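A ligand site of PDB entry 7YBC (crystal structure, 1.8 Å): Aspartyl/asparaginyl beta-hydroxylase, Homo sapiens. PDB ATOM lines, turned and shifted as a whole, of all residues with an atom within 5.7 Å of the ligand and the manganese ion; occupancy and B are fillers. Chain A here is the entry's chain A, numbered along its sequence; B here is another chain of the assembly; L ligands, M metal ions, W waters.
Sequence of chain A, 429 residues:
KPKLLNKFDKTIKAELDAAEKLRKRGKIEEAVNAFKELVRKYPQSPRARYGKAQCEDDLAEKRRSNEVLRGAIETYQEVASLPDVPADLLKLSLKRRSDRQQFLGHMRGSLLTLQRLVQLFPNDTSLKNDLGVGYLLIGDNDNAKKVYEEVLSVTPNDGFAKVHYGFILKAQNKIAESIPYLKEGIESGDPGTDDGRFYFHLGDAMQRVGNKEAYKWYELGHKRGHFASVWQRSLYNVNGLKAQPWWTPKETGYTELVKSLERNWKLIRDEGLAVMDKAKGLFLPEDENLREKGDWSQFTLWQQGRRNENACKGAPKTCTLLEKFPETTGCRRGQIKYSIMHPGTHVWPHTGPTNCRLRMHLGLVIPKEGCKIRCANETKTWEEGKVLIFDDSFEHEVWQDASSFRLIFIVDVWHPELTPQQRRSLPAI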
ATOM      1  N   LEU A 290     -21.476  32.549 -11.951  1.00  0.00           N
ATOM      2  CA  LEU A 290     -21.023  31.191 -12.241  1.00  0.00           C
ATOM      3  C   LEU A 290     -19.926  30.690 -11.297  1.00  0.00           C
ATOM      4  O   LEU A 290     -19.568  29.502 -11.380  1.00  0.00           O
ATOM      5  CB  LEU A 290     -20.527  31.100 -13.680  1.00  0.00           C
ATOM      6  CG  LEU A 290     -21.535  31.391 -14.789  1.00  0.00           C
ATOM      7  CD1 LEU A 290     -20.846  31.367 -16.155  1.00  0.00           C
ATOM      8  CD2 LEU A 290     -22.664  30.389 -14.760  1.00  0.00           C
ATOM      9  N   TRP A 296     -11.853  35.410 -11.495  1.00  0.00           N
ATOM     10  CA  TRP A 296     -11.965  35.000 -12.896  1.00  0.00           C
ATOM     11  C   TRP A 296     -12.441  36.227 -13.656  1.00  0.00           C
ATOM     12  O   TRP A 296     -13.460  36.823 -13.281  1.00  0.00           O
ATOM     13  CB  TRP A 296     -12.928  33.824 -13.023  1.00  0.00           C
ATOM     14  CG  TRP A 296     -13.358  33.443 -14.396  1.00  0.00           C
ATOM     15  CD1 TRP A 296     -12.683  33.640 -15.570  1.00  0.00           C
ATOM     16  CD2 TRP A 296     -14.589  32.792 -14.736  1.00  0.00           C
ATOM     17  NE1 TRP A 296     -13.434  33.154 -16.623  1.00  0.00           N
ATOM     18  CE2 TRP A 296     -14.600  32.624 -16.136  1.00  0.00           C
ATOM     19  CE3 TRP A 296     -15.676  32.327 -13.990  1.00  0.00           C
ATOM     20  CZ2 TRP A 296     -15.665  32.028 -16.811  1.00  0.00           C
ATOM     21  CZ3 TRP A 296     -16.731  31.722 -14.661  1.00  0.00           C
ATOM     22  CH2 TRP A 296     -16.716  31.569 -16.047  1.00  0.00           C
ATOM     23  N   GLN A 298     -12.351  38.330 -17.804  1.00  0.00           N
ATOM     24  CA  GLN A 298     -12.258  38.143 -19.246  1.00  0.00           C
ATOM     25  C   GLN A 298     -12.077  39.487 -19.954  1.00  0.00           C
ATOM     26  O   GLN A 298     -12.623  40.508 -19.521  1.00  0.00           O
ATOM     27  CB  GLN A 298     -13.500  37.389 -19.763  1.00  0.00           C
ATOM     28  CG  GLN A 298     -13.652  36.018 -19.082  1.00  0.00           C
ATOM     29  CD  GLN A 298     -14.874  35.223 -19.487  1.00  0.00           C
ATOM     30  OE1 GLN A 298     -14.764  34.088 -19.947  1.00  0.00           O
ATOM     31  NE2 GLN A 298     -16.057  35.797 -19.287  1.00  0.00           N
ATOM     32  N   SER A 339      -9.219  34.773 -21.030  1.00  0.00           N
ATOM     33  CA  SER A 339      -9.817  34.437 -19.734  1.00  0.00           C
ATOM     34  C   SER A 339      -8.704  34.103 -18.747  1.00  0.00           C
ATOM     35  O   SER A 339      -7.956  33.149 -18.965  1.00  0.00           O
ATOM     36  CB  SER A 339     -10.792  33.262 -19.853  1.00  0.00           C
ATOM     37  OG  SER A 339     -11.404  32.993 -18.611  1.00  0.00           O
ATOM     38  N   ILE A 340      -8.625  34.879 -17.668  1.00  0.00           N
ATOM     39  CA  ILE A 340      -7.653  34.646 -16.606  1.00  0.00           C
ATOM     40  C   ILE A 340      -8.401  34.119 -15.382  1.00  0.00           C
ATOM     41  O   ILE A 340      -9.476  34.602 -15.032  1.00  0.00           O
ATOM     42  CB  ILE A 340      -6.860  35.918 -16.272  1.00  0.00           C
ATOM     43  CG1 ILE A 340      -5.695  35.573 -15.333  1.00  0.00           C
ATOM     44  CG2 ILE A 340      -7.738  36.970 -15.623  1.00  0.00           C
ATOM     45  CD1 ILE A 340      -4.677  36.691 -15.197  1.00  0.00           C
ATOM     46  N   MET A 341      -7.810  33.096 -14.756  1.00  0.00           N
ATOM     47  CA  MET A 341      -8.380  32.483 -13.558  1.00  0.00           C
ATOM     48  C   MET A 341      -7.258  32.237 -12.560  1.00  0.00           C
ATOM     49  O   MET A 341      -6.181  31.770 -12.924  1.00  0.00           O
ATOM     50  CB  MET A 341      -9.084  31.161 -13.898  1.00  0.00           C
ATOM     51  CG  MET A 341      -9.932  30.614 -12.768  1.00  0.00           C
ATOM     52  SD  MET A 341     -10.828  29.118 -13.185  1.00  0.00           S
ATOM     53  CE  MET A 341     -11.910  29.743 -14.468  1.00  0.00           C
ATOM     54  N   VAL A 347     -15.576  27.077 -10.583  1.00  0.00           N
ATOM     55  CA  VAL A 347     -16.701  27.485 -11.412  1.00  0.00           C
ATOM     56  C   VAL A 347     -17.774  26.408 -11.327  1.00  0.00           C
ATOM     57  O   VAL A 347     -17.508  25.245 -11.643  1.00  0.00           O
ATOM     58  CB  VAL A 347     -16.259  27.678 -12.869  1.00  0.00           C
ATOM     59  CG1 VAL A 347     -17.449  28.048 -13.758  1.00  0.00           C
ATOM     60  CG2 VAL A 347     -15.159  28.721 -12.970  1.00  0.00           C
ATOM     61  N   HIS A 350     -22.173  24.291 -15.198  1.00  0.00           N
ATOM     62  CA  HIS A 350     -23.069  25.174 -15.917  1.00  0.00           C
ATOM     63  C   HIS A 350     -23.085  24.798 -17.389  1.00  0.00           C
ATOM     64  O   HIS A 350     -22.262  24.020 -17.871  1.00  0.00           O
ATOM     65  CB  HIS A 350     -22.682  26.658 -15.746  1.00  0.00           C
ATOM     66  CG  HIS A 350     -21.395  27.013 -16.421  1.00  0.00           C
ATOM     67  ND1 HIS A 350     -20.156  26.698 -15.898  1.00  0.00           N
ATOM     68  CD2 HIS A 350     -21.149  27.680 -17.578  1.00  0.00           C
ATOM     69  CE1 HIS A 350     -19.207  27.132 -16.704  1.00  0.00           C
ATOM     70  NE2 HIS A 350     -19.776  27.726 -17.740  1.00  0.00           N
ATOM     71  N   ARG A 359     -16.625  25.746 -28.696  1.00  0.00           N
ATOM     72  CA  ARG A 359     -15.719  26.629 -27.980  1.00  0.00           C
ATOM     73  C   ARG A 359     -14.312  26.061 -28.038  1.00  0.00           C
ATOM     74  O   ARG A 359     -14.080  24.933 -27.604  1.00  0.00           O
ATOM     75  CB  ARG A 359     -16.193  26.787 -26.531  1.00  0.00           C
ATOM     76  CG  ARG A 359     -15.607  27.929 -25.787  1.00  0.00           C
ATOM     77  CD  ARG A 359     -16.605  28.423 -24.748  1.00  0.00           C
ATOM     78  NE  ARG A 359     -17.283  29.638 -25.161  1.00  0.00           N
ATOM     79  CZ  ARG A 359     -17.856  30.493 -24.325  1.00  0.00           C
ATOM     80  NH1 ARG A 359     -17.824  30.230 -23.016  1.00  0.00           N
ATOM     81  NH2 ARG A 359     -18.444  31.588 -24.768  1.00  0.00           N
ATOM     82  N   HIS A 361     -10.388  26.483 -26.729  1.00  0.00           N
ATOM     83  CA  HIS A 361      -9.486  27.050 -25.735  1.00  0.00           C
ATOM     84  C   HIS A 361      -8.049  26.873 -26.214  1.00  0.00           C
ATOM     85  O   HIS A 361      -7.652  25.752 -26.540  1.00  0.00           O
ATOM     86  CB  HIS A 361      -9.617  26.346 -24.388  1.00  0.00           C
ATOM     87  CG  HIS A 361     -10.849  26.696 -23.615  1.00  0.00           C
ATOM     88  ND1 HIS A 361     -11.093  26.193 -22.353  1.00  0.00           N
ATOM     89  CD2 HIS A 361     -11.890  27.509 -23.904  1.00  0.00           C
ATOM     90  CE1 HIS A 361     -12.242  26.672 -21.904  1.00  0.00           C
ATOM     91  NE2 HIS A 361     -12.742  27.467 -22.829  1.00  0.00           N
ATOM     92  N   ILE A 373     -10.617  21.081 -16.440  1.00  0.00           N
ATOM     93  CA  ILE A 373     -11.971  21.370 -16.899  1.00  0.00           C
ATOM     94  C   ILE A 373     -12.676  20.051 -17.188  1.00  0.00           C
ATOM     95  O   ILE A 373     -12.124  19.193 -17.889  1.00  0.00           O
ATOM     96  CB  ILE A 373     -11.982  22.262 -18.153  1.00  0.00           C
ATOM     97  CG1 ILE A 373     -13.406  22.353 -18.715  1.00  0.00           C
ATOM     98  CG2 ILE A 373     -11.027  21.729 -19.214  1.00  0.00           C
ATOM     99  CD1 ILE A 373     -13.583  23.421 -19.771  1.00  0.00           C
ATOM    100  N   TRP A 382      -5.334  21.763 -19.822  1.00  0.00           N
ATOM    101  CA  TRP A 382      -4.815  22.598 -20.892  1.00  0.00           C
ATOM    102  C   TRP A 382      -3.312  22.385 -21.066  1.00  0.00           C
ATOM    103  O   TRP A 382      -2.617  21.938 -20.145  1.00  0.00           O
ATOM    104  CB  TRP A 382      -5.080  24.082 -20.621  1.00  0.00           C
ATOM    105  CG  TRP A 382      -6.513  24.466 -20.550  1.00  0.00           C
ATOM    106  CD1 TRP A 382      -7.325  24.803 -21.589  1.00  0.00           C
ATOM    107  CD2 TRP A 382      -7.310  24.578 -19.375  1.00  0.00           C
ATOM    108  NE1 TRP A 382      -8.583  25.114 -21.133  1.00  0.00           N
ATOM    109  CE2 TRP A 382      -8.596  24.979 -19.773  1.00  0.00           C
ATOM    110  CE3 TRP A 382      -7.050  24.378 -18.013  1.00  0.00           C
ATOM    111  CZ2 TRP A 382      -9.631  25.168 -18.852  1.00  0.00           C
ATOM    112  CZ3 TRP A 382      -8.070  24.563 -17.108  1.00  0.00           C
ATOM    113  CH2 TRP A 382      -9.339  24.957 -17.532  1.00  0.00           C
ATOM    114  N   PHE A 390     -14.527  21.985 -27.098  1.00  0.00           N
ATOM    115  CA  PHE A 390     -15.663  21.322 -26.460  1.00  0.00           C
ATOM    116  C   PHE A 390     -16.935  22.064 -26.831  1.00  0.00           C
ATOM    117  O   PHE A 390     -16.912  23.208 -27.311  1.00  0.00           O
ATOM    118  CB  PHE A 390     -15.471  21.230 -24.932  1.00  0.00           C
ATOM    119  CG  PHE A 390     -15.557  22.546 -24.205  1.00  0.00           C
ATOM    120  CD1 PHE A 390     -14.522  23.457 -24.286  1.00  0.00           C
ATOM    121  CD2 PHE A 390     -16.654  22.842 -23.414  1.00  0.00           C
ATOM    122  CE1 PHE A 390     -14.593  24.662 -23.621  1.00  0.00           C
ATOM    123  CE2 PHE A 390     -16.738  24.049 -22.742  1.00  0.00           C
ATOM    124  CZ  PHE A 390     -15.705  24.951 -22.854  1.00  0.00           C
ATOM    125  N   ASP A 392     -19.924  23.709 -25.231  1.00  0.00           N
ATOM    126  CA  ASP A 392     -20.277  24.237 -23.918  1.00  0.00           C
ATOM    127  C   ASP A 392     -21.777  24.271 -23.682  1.00  0.00           C
ATOM    128  O   ASP A 392     -22.219  24.743 -22.633  1.00  0.00           O
ATOM    129  CB  ASP A 392     -19.634  25.628 -23.698  1.00  0.00           C
ATOM    130  CG  ASP A 392     -20.449  26.797 -24.262  1.00  0.00           C
ATOM    131  OD1 ASP A 392     -21.041  26.688 -25.356  1.00  0.00           O
ATOM    132  OD2 ASP A 392     -20.456  27.859 -23.594  1.00  0.00           O
ATOM    133  N   HIS A 396     -20.484  21.705 -17.930  1.00  0.00           N
ATOM    134  CA  HIS A 396     -19.043  21.718 -17.702  1.00  0.00           C
ATOM    135  C   HIS A 396     -18.705  22.526 -16.459  1.00  0.00           C
ATOM    136  O   HIS A 396     -19.524  23.301 -15.954  1.00  0.00           O
ATOM    137  CB  HIS A 396     -18.297  22.246 -18.960  1.00  0.00           C
ATOM    138  CG  HIS A 396     -18.754  23.594 -19.406  1.00  0.00           C
ATOM    139  ND1 HIS A 396     -19.935  23.793 -20.085  1.00  0.00           N
ATOM    140  CD2 HIS A 396     -18.178  24.812 -19.273  1.00  0.00           C
ATOM    141  CE1 HIS A 396     -20.081  25.089 -20.341  1.00  0.00           C
ATOM    142  NE2 HIS A 396     -19.025  25.724 -19.860  1.00  0.00           N
ATOM    143  N   VAL A 398     -15.075  23.896 -13.863  1.00  0.00           N
ATOM    144  CA  VAL A 398     -13.663  24.265 -13.879  1.00  0.00           C
ATOM    145  C   VAL A 398     -13.143  24.482 -12.470  1.00  0.00           C
ATOM    146  O   VAL A 398     -13.866  24.979 -11.595  1.00  0.00           O
ATOM    147  CB  VAL A 398     -13.415  25.513 -14.747  1.00  0.00           C
ATOM    148  CG1 VAL A 398     -11.945  25.909 -14.714  1.00  0.00           C
ATOM    149  CG2 VAL A 398     -13.863  25.251 -16.180  1.00  0.00           C
ATOM    150  N   ARG A 406      -3.594  31.392 -14.377  1.00  0.00           N
ATOM    151  CA  ARG A 406      -3.831  30.572 -15.559  1.00  0.00           C
ATOM    152  C   ARG A 406      -4.526  31.431 -16.605  1.00  0.00           C
ATOM    153  O   ARG A 406      -5.638  31.924 -16.364  1.00  0.00           O
ATOM    154  CB  ARG A 406      -4.699  29.360 -15.234  1.00  0.00           C
ATOM    155  CG  ARG A 406      -4.956  28.408 -16.406  1.00  0.00           C
ATOM    156  CD  ARG A 406      -6.451  28.152 -16.570  1.00  0.00           C
ATOM    157  NE  ARG A 406      -7.158  29.386 -16.910  1.00  0.00           N
ATOM    158  CZ  ARG A 406      -8.461  29.468 -17.150  1.00  0.00           C
ATOM    159  NH1 ARG A 406      -9.220  28.385 -17.079  1.00  0.00           N
ATOM    160  NH2 ARG A 406      -9.006  30.635 -17.452  1.00  0.00           N
ATOM    161  N   ILE A 408      -5.910  31.584 -20.625  1.00  0.00           N
ATOM    162  CA  ILE A 408      -6.270  30.909 -21.868  1.00  0.00           C
ATOM    163  C   ILE A 408      -6.890  31.925 -22.810  1.00  0.00           C
ATOM    164  O   ILE A 408      -7.282  33.024 -22.412  1.00  0.00           O
ATOM    165  CB  ILE A 408      -7.227  29.725 -21.659  1.00  0.00           C
ATOM    166  CG1 ILE A 408      -8.590  30.190 -21.123  1.00  0.00           C
ATOM    167  CG2 ILE A 408      -6.633  28.696 -20.689  1.00  0.00           C
ATOM    168  CD1 ILE A 408      -9.601  29.079 -20.980  1.00  0.00           C
ATOM    169  N   ILE A 410     -10.002  32.159 -25.630  1.00  0.00           N
ATOM    170  CA  ILE A 410     -11.254  31.480 -25.957  1.00  0.00           C
ATOM    171  C   ILE A 410     -11.753  31.979 -27.302  1.00  0.00           C
ATOM    172  O   ILE A 410     -11.913  33.185 -27.504  1.00  0.00           O
ATOM    173  CB  ILE A 410     -12.322  31.697 -24.859  1.00  0.00           C
ATOM    174  CG1 ILE A 410     -11.800  31.178 -23.513  1.00  0.00           C
ATOM    175  CG2 ILE A 410     -13.620  31.009 -25.249  1.00  0.00           C
ATOM    176  CD1 ILE A 410     -12.808  31.259 -22.352  1.00  0.00           C
ATOM    177  N   ASP B  18     -21.639  33.204 -21.193  1.00  0.00           N
ATOM    178  CA  ASP B  18     -21.229  31.867 -20.815  1.00  0.00           C
ATOM    179  C   ASP B  18     -22.349  31.026 -20.220  1.00  0.00           C
ATOM    180  O   ASP B  18     -22.221  29.793 -20.178  1.00  0.00           O
ATOM    181  CB  ASP B  18     -20.083  31.952 -19.786  1.00  0.00           C
ATOM    182  CG  ASP B  18     -18.880  32.673 -20.338  1.00  0.00           C
ATOM    183  OD1 ASP B  18     -18.464  32.326 -21.460  1.00  0.00           O
ATOM    184  OD2 ASP B  18     -18.361  33.588 -19.655  1.00  0.00           O
HETATM  185  C1  LIG L   1     -15.932  28.224 -20.929  1.00  0.00           C
HETATM  186  C2  LIG L   1     -15.608  28.004 -19.610  1.00  0.00           C
HETATM  187  C3  LIG L   1     -14.136  28.050 -19.265  1.00  0.00           C
HETATM  188  C4  LIG L   1     -13.769  29.208 -18.336  1.00  0.00           C
HETATM  189  C5  LIG L   1     -12.286  29.100 -18.021  1.00  0.00           C
HETATM  190  C6  LIG L   1     -14.528  29.187 -17.008  1.00  0.00           C
HETATM  191  O1  LIG L   1     -17.212  28.105 -21.364  1.00  0.00           O
HETATM  192  O2  LIG L   1     -15.096  28.520 -21.768  1.00  0.00           O
HETATM  193  O3  LIG L   1     -16.449  27.818 -18.749  1.00  0.00           O
HETATM  194  O4  LIG L   1     -14.016  30.433 -19.015  1.00  0.00           O
HETATM  195  O5  LIG L   1     -11.671  30.288 -18.223  1.00  0.00           O
HETATM  196  O6  LIG L   1     -11.708  28.106 -17.663  1.00  0.00           O
HETATM  197 MN    MN M   1     -18.517  27.899 -19.645  1.00  0.00          MN
HETATM  198  O   HOH W   1     -15.792  31.490 -20.682  1.00  0.00           O
HETATM  199  O   HOH W   2     -17.710  30.135 -19.102  1.00  0.00           O
HETATM  200  O   HOH W   3     -20.207  28.413 -20.926  1.00  0.00           O
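The guanidinium group of Arg 406 lies within hydrogen-bond range of the backbone carbonyl oxygen of Ser 339 (3.1 Å). N of Met 341 sits at hydrogen-bond distance from O of Arg 406. The backbone NH (N) of Ser 339 sits at hydrogen-bond distance from the backbone carbonyl oxygen (O) of Ile 408. The backbone NH (N) of Arg 359 is in hydrogen-bond range of the backbone carbonyl oxygen (O) of Phe 390 (2.9 Å). OD2 of Asp 392 lies within salt-bridge range of NH1 of Arg 359, 3.6 Å away. The guanidinium group of Arg 359 lies within salt-bridge range of the side-chain carboxylate of Asp 18 of chain B, 2.7 Å away. A ring nitrogen (ND1) of His 361 lies within hydrogen-bond range of the indole nitrogen (NE1) of Trp 382, at 3.0 Å. The side-chain amide nitrogen (NE2) of Gln 298 lies within hydrogen-bond range of the side-chain carboxylate (OD2) of Asp 18 of chain B (3.2 Å).
Water W3 lies within hydrogen-bond range of the backbone carbonyl oxygen of Asp 18 of chain B (2.6 Å) and the side-chain carboxylate of Asp 392 (2.7 Å). Water W1 lies within hydrogen-bond range of O4 of the ligand (2.7 Å), OE1 of Gln 298 (2.9 Å), OD1 of Asp 18 of chain B (2.9 Å) and NH1 of Arg 359 (3.3 Å).
The guanidinium group of Arg 406 lies within salt-bridge range of an oxygen (O6) of the ligand. An oxygen (O5) of the ligand sits at hydrogen-bond distance from the side-chain hydroxyl of Ser 339, 2.7 Å away. NH1 of Arg 359 is in salt-bridge range of O2 of the ligand (3.5 Å). A ring nitrogen (NE2) of His 361 is in hydrogen-bond range of an oxygen (O2) of the ligand, 2.8 Å away.
Of the 20 residues printed, 2 come within 4 Å of the manganese ion. The nearest printed residue that does not touch the manganese ion is Arg 359 (4.2 Å).
The manganese ion is bound by O1 of the ligand, 2.2 Å away. The manganese ion is bound by water W3 (2.2 Å). The manganese ion is bound by a ring nitrogen (NE2) of His 396, 2.2 Å away. An oxygen (O3) of the ligand binds the manganese ion (2.3 Å). The manganese ion is bound by NE2 of His 350 (2.3 Å). Water W2 is bound to the manganese ion, at 2.4 Å.
Trp 296 touches the ligand. Gln 298 touches the ligand. Met 341 touches the ligand. CZ2 of Trp 382 touches O6 of the ligand, at 3.8 Å. Phe 390 touches the ligand (CZ to O2, 3.8 Å). Asp 392 touches the ligand (OD2 to O1, 3.9 Å). Val 398 touches the ligand. CD1 of Ile 408 touches O5 of the ligand, at 3.7 Å. CD1 of Ile 410 touches O2 of the ligand (3.6 Å). Of the 20 residues printed, 15 come within 4 Å of the ligand. The nearest printed residue that does not touch the ligand is Val 347 (4.1 Å).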
